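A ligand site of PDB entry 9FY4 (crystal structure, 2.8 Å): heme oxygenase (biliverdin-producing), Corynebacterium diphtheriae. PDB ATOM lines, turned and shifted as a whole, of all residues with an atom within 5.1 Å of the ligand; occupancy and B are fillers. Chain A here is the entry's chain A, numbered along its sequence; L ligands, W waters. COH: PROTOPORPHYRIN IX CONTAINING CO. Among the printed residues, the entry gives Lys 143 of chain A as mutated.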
ATOM      1  N   ALA A   9     -13.333 -15.019 -17.569  1.00  0.00           N
ATOM      2  CA  ALA A   9     -13.778 -15.035 -16.185  1.00  0.00           C
ATOM      3  C   ALA A   9     -13.361 -16.324 -15.472  1.00  0.00           C
ATOM      4  O   ALA A   9     -12.918 -16.267 -14.323  1.00  0.00           O
ATOM      5  CB  ALA A   9     -15.288 -14.865 -16.116  1.00  0.00           C
ATOM      6  N   LYS A  13     -10.303 -16.957 -12.400  1.00  0.00           N
ATOM      7  CA  LYS A  13     -10.586 -17.663 -11.152  1.00  0.00           C
ATOM      8  C   LYS A  13      -9.716 -18.909 -10.948  1.00  0.00           C
ATOM      9  O   LYS A  13      -9.569 -19.374  -9.820  1.00  0.00           O
ATOM     10  CB  LYS A  13     -12.076 -18.003 -11.032  1.00  0.00           C
ATOM     11  CG  LYS A  13     -12.589 -18.011  -9.594  1.00  0.00           C
ATOM     12  CD  LYS A  13     -13.949 -18.652  -9.459  1.00  0.00           C
ATOM     13  CE  LYS A  13     -14.398 -18.737  -8.017  1.00  0.00           C
ATOM     14  NZ  LYS A  13     -15.630 -19.540  -7.863  1.00  0.00           N
ATOM     15  N   HIS A  20      -5.036 -16.275  -4.325  1.00  0.00           N
ATOM     16  CA  HIS A  20      -6.208 -15.992  -3.491  1.00  0.00           C
ATOM     17  C   HIS A  20      -6.142 -16.766  -2.166  1.00  0.00           C
ATOM     18  O   HIS A  20      -6.593 -16.254  -1.143  1.00  0.00           O
ATOM     19  CB  HIS A  20      -7.497 -16.295  -4.266  1.00  0.00           C
ATOM     20  CG  HIS A  20      -8.741 -16.160  -3.454  1.00  0.00           C
ATOM     21  ND1 HIS A  20      -9.495 -17.260  -3.094  1.00  0.00           N
ATOM     22  CD2 HIS A  20      -9.328 -15.047  -2.943  1.00  0.00           C
ATOM     23  CE1 HIS A  20     -10.506 -16.785  -2.397  1.00  0.00           C
ATOM     24  NE2 HIS A  20     -10.447 -15.460  -2.281  1.00  0.00           N
ATOM     25  N   ALA A  23      -3.808 -14.932   0.324  1.00  0.00           N
ATOM     26  CA  ALA A  23      -4.372 -13.724   0.927  1.00  0.00           C
ATOM     27  C   ALA A  23      -5.206 -14.031   2.169  1.00  0.00           C
ATOM     28  O   ALA A  23      -5.095 -13.332   3.177  1.00  0.00           O
ATOM     29  CB  ALA A  23      -5.218 -12.977  -0.102  1.00  0.00           C
ATOM     30  N   GLU A  24      -6.033 -15.090   2.115  1.00  0.00           N
ATOM     31  CA  GLU A  24      -6.852 -15.470   3.259  1.00  0.00           C
ATOM     32  C   GLU A  24      -6.058 -16.182   4.373  1.00  0.00           C
ATOM     33  O   GLU A  24      -6.525 -16.251   5.507  1.00  0.00           O
ATOM     34  CB  GLU A  24      -8.076 -16.300   2.824  1.00  0.00           C
ATOM     35  CG  GLU A  24      -7.752 -17.458   1.896  1.00  0.00           C
ATOM     36  CD  GLU A  24      -8.958 -18.138   1.285  1.00  0.00           C
ATOM     37  OE1 GLU A  24      -9.952 -18.348   2.015  1.00  0.00           O
ATOM     38  OE2 GLU A  24      -8.914 -18.461   0.074  1.00  0.00           O
ATOM     39  N   MET A  29      -5.204 -11.016   8.365  1.00  0.00           N
ATOM     40  CA  MET A  29      -6.568 -11.372   7.992  1.00  0.00           C
ATOM     41  C   MET A  29      -7.103 -12.526   8.836  1.00  0.00           C
ATOM     42  O   MET A  29      -8.272 -12.510   9.204  1.00  0.00           O
ATOM     43  CB  MET A  29      -6.669 -11.688   6.496  1.00  0.00           C
ATOM     44  CG  MET A  29      -7.120 -10.508   5.666  1.00  0.00           C
ATOM     45  SD  MET A  29      -8.791  -9.941   6.078  1.00  0.00           S
ATOM     46  CE  MET A  29      -9.517  -9.891   4.468  1.00  0.00           C
ATOM     47  N   LEU A  33     -10.450 -11.849  11.194  1.00  0.00           N
ATOM     48  CA  LEU A  33     -11.668 -12.628  11.026  1.00  0.00           C
ATOM     49  C   LEU A  33     -11.942 -13.566  12.210  1.00  0.00           C
ATOM     50  O   LEU A  33     -13.092 -13.890  12.478  1.00  0.00           O
ATOM     51  CB  LEU A  33     -11.630 -13.395   9.701  1.00  0.00           C
ATOM     52  CG  LEU A  33     -11.402 -12.548   8.454  1.00  0.00           C
ATOM     53  CD1 LEU A  33     -11.301 -13.417   7.234  1.00  0.00           C
ATOM     54  CD2 LEU A  33     -12.478 -11.503   8.275  1.00  0.00           C
ATOM     55  N   TYR A 130     -11.419  -6.533 -11.370  1.00  0.00           N
ATOM     56  CA  TYR A 130     -11.827  -7.898 -11.035  1.00  0.00           C
ATOM     57  C   TYR A 130     -11.388  -8.253  -9.610  1.00  0.00           C
ATOM     58  O   TYR A 130     -12.222  -8.681  -8.806  1.00  0.00           O
ATOM     59  CB  TYR A 130     -11.275  -8.907 -12.082  1.00  0.00           C
ATOM     60  CG  TYR A 130     -11.221 -10.340 -11.613  1.00  0.00           C
ATOM     61  CD1 TYR A 130     -12.376 -11.083 -11.444  1.00  0.00           C
ATOM     62  CD2 TYR A 130     -10.008 -10.946 -11.310  1.00  0.00           C
ATOM     63  CE1 TYR A 130     -12.339 -12.403 -11.002  1.00  0.00           C
ATOM     64  CE2 TYR A 130      -9.962 -12.261 -10.840  1.00  0.00           C
ATOM     65  CZ  TYR A 130     -11.122 -12.990 -10.704  1.00  0.00           C
ATOM     66  OH  TYR A 130     -11.075 -14.280 -10.261  1.00  0.00           O
ATOM     67  N   VAL A 131     -10.096  -8.069  -9.307  1.00  0.00           N
ATOM     68  CA  VAL A 131      -9.521  -8.402  -7.998  1.00  0.00           C
ATOM     69  C   VAL A 131     -10.268  -7.735  -6.849  1.00  0.00           C
ATOM     70  O   VAL A 131     -10.648  -8.415  -5.894  1.00  0.00           O
ATOM     71  CB  VAL A 131      -7.995  -8.106  -7.981  1.00  0.00           C
ATOM     72  CG1 VAL A 131      -7.435  -8.064  -6.558  1.00  0.00           C
ATOM     73  CG2 VAL A 131      -7.248  -9.134  -8.822  1.00  0.00           C
ATOM     74  N   ARG A 132     -10.531  -6.416  -6.943  1.00  0.00           N
ATOM     75  CA  ARG A 132     -11.187  -5.712  -5.854  1.00  0.00           C
ATOM     76  C   ARG A 132     -12.719  -5.807  -5.843  1.00  0.00           C
ATOM     77  O   ARG A 132     -13.262  -6.304  -4.858  1.00  0.00           O
ATOM     78  CB  ARG A 132     -10.740  -4.236  -5.794  1.00  0.00           C
ATOM     79  CG  ARG A 132      -9.312  -4.031  -5.263  1.00  0.00           C
ATOM     80  CD  ARG A 132      -9.012  -4.744  -3.944  1.00  0.00           C
ATOM     81  NE  ARG A 132      -9.987  -4.438  -2.904  1.00  0.00           N
ATOM     82  CZ  ARG A 132     -10.104  -5.105  -1.763  1.00  0.00           C
ATOM     83  NH1 ARG A 132      -9.294  -6.116  -1.488  1.00  0.00           N
ATOM     84  NH2 ARG A 132     -11.034  -4.756  -0.875  1.00  0.00           N
ATOM     85  N   LEU A 134     -15.085  -7.712  -7.609  1.00  0.00           N
ATOM     86  CA  LEU A 134     -15.751  -9.029  -7.582  1.00  0.00           C
ATOM     87  C   LEU A 134     -15.625  -9.712  -6.220  1.00  0.00           C
ATOM     88  O   LEU A 134     -16.547 -10.403  -5.787  1.00  0.00           O
ATOM     89  CB  LEU A 134     -15.319  -9.944  -8.735  1.00  0.00           C
ATOM     90  CG  LEU A 134     -16.270 -11.123  -9.056  1.00  0.00           C
ATOM     91  CD1 LEU A 134     -17.682 -10.641  -9.319  1.00  0.00           C
ATOM     92  CD2 LEU A 134     -15.784 -11.900 -10.243  1.00  0.00           C
ATOM     93  N   GLY A 135     -14.495  -9.493  -5.535  1.00  0.00           N
ATOM     94  CA  GLY A 135     -14.274 -10.022  -4.194  1.00  0.00           C
ATOM     95  C   GLY A 135     -15.166  -9.349  -3.179  1.00  0.00           C
ATOM     96  O   GLY A 135     -15.604  -9.981  -2.214  1.00  0.00           O
ATOM     97  N   SER A 138     -18.854 -10.781  -3.590  1.00  0.00           N
ATOM     98  CA  SER A 138     -19.015 -12.167  -3.164  1.00  0.00           C
ATOM     99  C   SER A 138     -18.708 -12.435  -1.689  1.00  0.00           C
ATOM    100  O   SER A 138     -19.178 -13.444  -1.155  1.00  0.00           O
ATOM    101  CB  SER A 138     -18.187 -13.099  -4.052  1.00  0.00           C
ATOM    102  OG  SER A 138     -16.856 -12.638  -4.173  1.00  0.00           O
ATOM    103  N   LYS A 143     -17.938 -10.679   5.695  1.00  0.00           N
ATOM    104  CA  LYS A 143     -17.021  -9.847   6.462  1.00  0.00           C
ATOM    105  C   LYS A 143     -17.751  -8.843   7.346  1.00  0.00           C
ATOM    106  O   LYS A 143     -17.310  -8.574   8.453  1.00  0.00           O
ATOM    107  CB  LYS A 143     -15.994  -9.176   5.544  1.00  0.00           C
ATOM    108  CG  LYS A 143     -15.037 -10.165   4.903  1.00  0.00           C
ATOM    109  CD  LYS A 143     -13.968  -9.494   4.056  1.00  0.00           C
ATOM    110  CE  LYS A 143     -14.548  -8.829   2.834  1.00  0.00           C
ATOM    111  NZ  LYS A 143     -13.495  -8.494   1.833  1.00  0.00           N
ATOM    112  N   LYS A 170     -26.447 -11.878  -6.345  1.00  0.00           N
ATOM    113  CA  LYS A 170     -25.953 -13.069  -7.024  1.00  0.00           C
ATOM    114  C   LYS A 170     -26.077 -12.940  -8.545  1.00  0.00           C
ATOM    115  O   LYS A 170     -25.179 -13.357  -9.280  1.00  0.00           O
ATOM    116  CB  LYS A 170     -26.673 -14.329  -6.526  1.00  0.00           C
ATOM    117  CG  LYS A 170     -26.196 -15.636  -7.176  1.00  0.00           C
ATOM    118  CD  LYS A 170     -24.718 -15.917  -6.900  1.00  0.00           C
ATOM    119  CE  LYS A 170     -23.968 -16.304  -8.148  1.00  0.00           C
ATOM    120  NZ  LYS A 170     -22.530 -16.575  -7.871  1.00  0.00           N
ATOM    121  N   LYS A 173     -23.188 -10.878  -9.973  1.00  0.00           N
ATOM    122  CA  LYS A 173     -21.912 -11.593 -10.090  1.00  0.00           C
ATOM    123  C   LYS A 173     -21.844 -12.326 -11.422  1.00  0.00           C
ATOM    124  O   LYS A 173     -20.818 -12.286 -12.086  1.00  0.00           O
ATOM    125  CB  LYS A 173     -21.731 -12.579  -8.935  1.00  0.00           C
ATOM    126  CG  LYS A 173     -21.837 -11.950  -7.549  1.00  0.00           C
ATOM    127  CD  LYS A 173     -21.792 -13.022  -6.470  1.00  0.00           C
ATOM    128  CE  LYS A 173     -22.297 -12.518  -5.135  1.00  0.00           C
ATOM    129  NZ  LYS A 173     -22.177 -13.546  -4.070  1.00  0.00           N
ATOM    130  N   ARG A 177     -19.326 -11.528 -14.657  1.00  0.00           N
ATOM    131  CA  ARG A 177     -18.498 -12.567 -15.276  1.00  0.00           C
ATOM    132  C   ARG A 177     -18.789 -12.699 -16.764  1.00  0.00           C
ATOM    133  O   ARG A 177     -17.873 -12.950 -17.537  1.00  0.00           O
ATOM    134  CB  ARG A 177     -18.664 -13.899 -14.547  1.00  0.00           C
ATOM    135  CG  ARG A 177     -18.087 -13.888 -13.145  1.00  0.00           C
ATOM    136  CD  ARG A 177     -18.636 -15.017 -12.302  1.00  0.00           C
ATOM    137  NE  ARG A 177     -18.655 -14.673 -10.878  1.00  0.00           N
ATOM    138  CZ  ARG A 177     -19.151 -15.453  -9.917  1.00  0.00           C
ATOM    139  NH1 ARG A 177     -19.683 -16.627 -10.223  1.00  0.00           N
ATOM    140  NH2 ARG A 177     -19.126 -15.059  -8.658  1.00  0.00           N
ATOM    141  N   PHE A 201      -3.180  -9.244  -6.796  1.00  0.00           N
ATOM    142  CA  PHE A 201      -3.368 -10.099  -5.625  1.00  0.00           C
ATOM    143  C   PHE A 201      -2.173  -9.973  -4.686  1.00  0.00           C
ATOM    144  O   PHE A 201      -2.339  -9.951  -3.470  1.00  0.00           O
ATOM    145  CB  PHE A 201      -3.584 -11.555  -6.038  1.00  0.00           C
ATOM    146  CG  PHE A 201      -5.035 -11.979  -6.034  1.00  0.00           C
ATOM    147  CD1 PHE A 201      -5.692 -12.257  -4.848  1.00  0.00           C
ATOM    148  CD2 PHE A 201      -5.735 -12.095  -7.222  1.00  0.00           C
ATOM    149  CE1 PHE A 201      -7.022 -12.635  -4.851  1.00  0.00           C
ATOM    150  CE2 PHE A 201      -7.077 -12.480  -7.220  1.00  0.00           C
ATOM    151  CZ  PHE A 201      -7.708 -12.742  -6.036  1.00  0.00           C
ATOM    152  N   ASN A 204      -2.451  -6.676  -2.700  1.00  0.00           N
ATOM    153  CA  ASN A 204      -3.393  -6.759  -1.583  1.00  0.00           C
ATOM    154  C   ASN A 204      -2.881  -7.634  -0.446  1.00  0.00           C
ATOM    155  O   ASN A 204      -3.177  -7.352   0.720  1.00  0.00           O
ATOM    156  CB  ASN A 204      -4.765  -7.217  -2.062  1.00  0.00           C
ATOM    157  CG  ASN A 204      -5.560  -6.107  -2.695  1.00  0.00           C
ATOM    158  OD1 ASN A 204      -6.237  -5.332  -2.022  1.00  0.00           O
ATOM    159  ND2 ASN A 204      -5.498  -6.018  -4.015  1.00  0.00           N
ATOM    160  N   PHE A 208      -1.808  -6.609   3.846  1.00  0.00           N
ATOM    161  CA  PHE A 208      -2.081  -7.367   5.069  1.00  0.00           C
ATOM    162  C   PHE A 208      -0.793  -7.710   5.810  1.00  0.00           C
ATOM    163  O   PHE A 208      -0.781  -7.715   7.034  1.00  0.00           O
ATOM    164  CB  PHE A 208      -2.846  -8.659   4.760  1.00  0.00           C
ATOM    165  CG  PHE A 208      -4.165  -8.448   4.055  1.00  0.00           C
ATOM    166  CD1 PHE A 208      -4.971  -7.372   4.369  1.00  0.00           C
ATOM    167  CD2 PHE A 208      -4.623  -9.348   3.110  1.00  0.00           C
ATOM    168  CE1 PHE A 208      -6.189  -7.177   3.729  1.00  0.00           C
ATOM    169  CE2 PHE A 208      -5.839  -9.161   2.482  1.00  0.00           C
ATOM    170  CZ  PHE A 208      -6.614  -8.074   2.783  1.00  0.00           C
HETATM  171 CO   COH L   1     -12.156 -13.706  -1.831  1.00  0.00          CO
HETATM  172  CHA COH L   1     -14.548 -14.342  -3.871  1.00  0.00           C
HETATM  173  CHB COH L   1     -10.247 -12.242  -4.040  1.00  0.00           C
HETATM  174  CHC COH L   1     -11.219 -11.863   0.656  1.00  0.00           C
HETATM  175  CHD COH L   1     -12.544 -16.452  -0.057  1.00  0.00           C
HETATM  176  NA  COH L   1     -12.369 -13.350  -3.679  1.00  0.00           N
HETATM  177  C1A COH L   1     -13.404 -13.661  -4.465  1.00  0.00           C
HETATM  178  C2A COH L   1     -13.302 -13.270  -5.891  1.00  0.00           C
HETATM  179  C3A COH L   1     -11.978 -12.618  -5.940  1.00  0.00           C
HETATM  180  C4A COH L   1     -11.526 -12.736  -4.533  1.00  0.00           C
HETATM  181  CMA COH L   1     -11.274 -11.994  -7.103  1.00  0.00           C
HETATM  182  CAA COH L   1     -14.293 -13.490  -7.001  1.00  0.00           C
HETATM  183  CBA COH L   1     -13.756 -14.623  -7.857  1.00  0.00           C
HETATM  184  CGA COH L   1     -14.837 -15.156  -8.755  1.00  0.00           C
HETATM  185  O1A COH L   1     -14.631 -15.221  -9.976  1.00  0.00           O
HETATM  186  O2A COH L   1     -15.897 -15.535  -8.228  1.00  0.00           O
HETATM  187  NB  COH L   1     -10.916 -12.277  -1.713  1.00  0.00           N
HETATM  188  C1B COH L   1     -10.147 -11.730  -2.679  1.00  0.00           C
HETATM  189  C2B COH L   1      -9.240 -10.618  -2.287  1.00  0.00           C
HETATM  190  C3B COH L   1      -9.555 -10.535  -0.860  1.00  0.00           C
HETATM  191  C4B COH L   1     -10.575 -11.576  -0.624  1.00  0.00           C
HETATM  192  CMB COH L   1      -8.293  -9.830  -3.157  1.00  0.00           C
HETATM  193  CAB COH L   1      -9.012  -9.627   0.183  1.00  0.00           C
HETATM  194  CBB COH L   1      -8.122  -8.702  -0.081  1.00  0.00           C
HETATM  195  NC  COH L   1     -11.911 -14.092   0.011  1.00  0.00           N
HETATM  196  C1C COH L   1     -11.519 -13.255   0.981  1.00  0.00           C
HETATM  197  C2C COH L   1     -11.404 -13.806   2.352  1.00  0.00           C
HETATM  198  C3C COH L   1     -11.804 -15.189   2.128  1.00  0.00           C
HETATM  199  C4C COH L   1     -12.091 -15.261   0.670  1.00  0.00           C
HETATM  200  CMC COH L   1     -10.998 -13.124   3.616  1.00  0.00           C
HETATM  201  CAC COH L   1     -11.886 -16.244   3.162  1.00  0.00           C
HETATM  202  CBC COH L   1     -12.823 -17.155   3.170  1.00  0.00           C
HETATM  203  ND  COH L   1     -13.366 -15.174  -1.952  1.00  0.00           N
HETATM  204  C1D COH L   1     -13.457 -16.267  -1.177  1.00  0.00           C
HETATM  205  C2D COH L   1     -14.516 -17.223  -1.548  1.00  0.00           C
HETATM  206  C3D COH L   1     -15.148 -16.597  -2.723  1.00  0.00           C
HETATM  207  C4D COH L   1     -14.349 -15.357  -2.846  1.00  0.00           C
HETATM  208  CMD COH L   1     -14.869 -18.532  -0.888  1.00  0.00           C
HETATM  209  CAD COH L   1     -16.302 -17.091  -3.540  1.00  0.00           C
HETATM  210  CBD COH L   1     -15.983 -17.212  -5.026  1.00  0.00           C
HETATM  211  CGD COH L   1     -17.286 -17.139  -5.795  1.00  0.00           C
HETATM  212  O1D COH L   1     -17.964 -16.102  -5.711  1.00  0.00           O
HETATM  213  O2D COH L   1     -17.629 -18.112  -6.485  1.00  0.00           O
HETATM  214  O   HOH W   1     -20.384 -18.448  -7.081  1.00  0.00           O
HETATM  215  O   HOH W   2     -13.619 -12.414  -1.161  1.00  0.00           O
HETATM  216  O   HOH W   3     -18.160 -19.090  -9.122  1.00  0.00           O
HETATM  217  O   HOH W   4     -20.675 -16.202  -5.572  1.00  0.00           O
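The guanidinium group (NH1) of Arg 132 lies within hydrogen-bond range of the side-chain amide oxygen (OD1) of Asn 204, 3.2 Å away. The side-chain hydroxyl (OG) of Ser 138 lies within hydrogen-bond range of the backbone carbonyl oxygen (O) of Leu 134 (2.8 Å). O of Lys 173 sits close to NE of Arg 177 (3.4 Å). A ring nitrogen (ND1) of His 20 lies close to the side-chain carboxylate (OE2) of Glu 24 (3.4 Å).
Water W4 lies within hydrogen-bond range of an oxygen (O1D) of the ligand (2.7 Å), the side-chain amino group of Lys 170 (3.0 Å) and the side-chain amino group of Lys 173 (3.4 Å). Water W1 bridges O2D of the ligand (2.8 Å) and NZ of Lys 170 (3.0 Å). Water W3 lies within hydrogen-bond range of the side-chain amino group (NZ) of Lys 13 (2.9 Å), an oxygen (O2D) of the ligand (2.9 Å) and the guanidinium group (NH1) of Arg 177 (3.1 Å).
Glu 24 touches the ligand (OE1 to CAC, 3.1 Å). Met 29 touches the ligand (CE to CMC, 3.7 Å). Leu 33 touches the ligand (CD1 to CMC, 3.6 Å). OH of Tyr 130 touches CBA of the ligand, 3.6 Å away. Val 131 touches the ligand (O to CMA, 3.8 Å). Arg 132 touches the ligand (NH1 to CBB, 3.2 Å). Leu 134 touches the ligand (CD2 to O1A, 3.5 Å). CA of Gly 135 touches C1A of the ligand, 3.8 Å away. OG of Ser 138 touches CHA of the ligand, at 2.9 Å. CZ of Phe 201 touches CHB of the ligand, 3.3 Å away. Phe 208 touches the ligand. Hydrophobic or aromatic side chains that line the ligand: His 20, Met 29, Leu 33, Tyr 130, Val 131, Leu 134, Phe 201 and Phe 208. Of the 20 residues printed, 14 come within 4 Å of the ligand.
An oxygen (O2A) of the ligand is in salt-bridge range of the guanidinium group of Arg 177 (3.3 Å). NE2 of His 20 is bound to CO of the ligand (2.5 Å). NZ of Lys 13 is in salt-bridge range of O2D of the ligand, 2.8 Å away.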
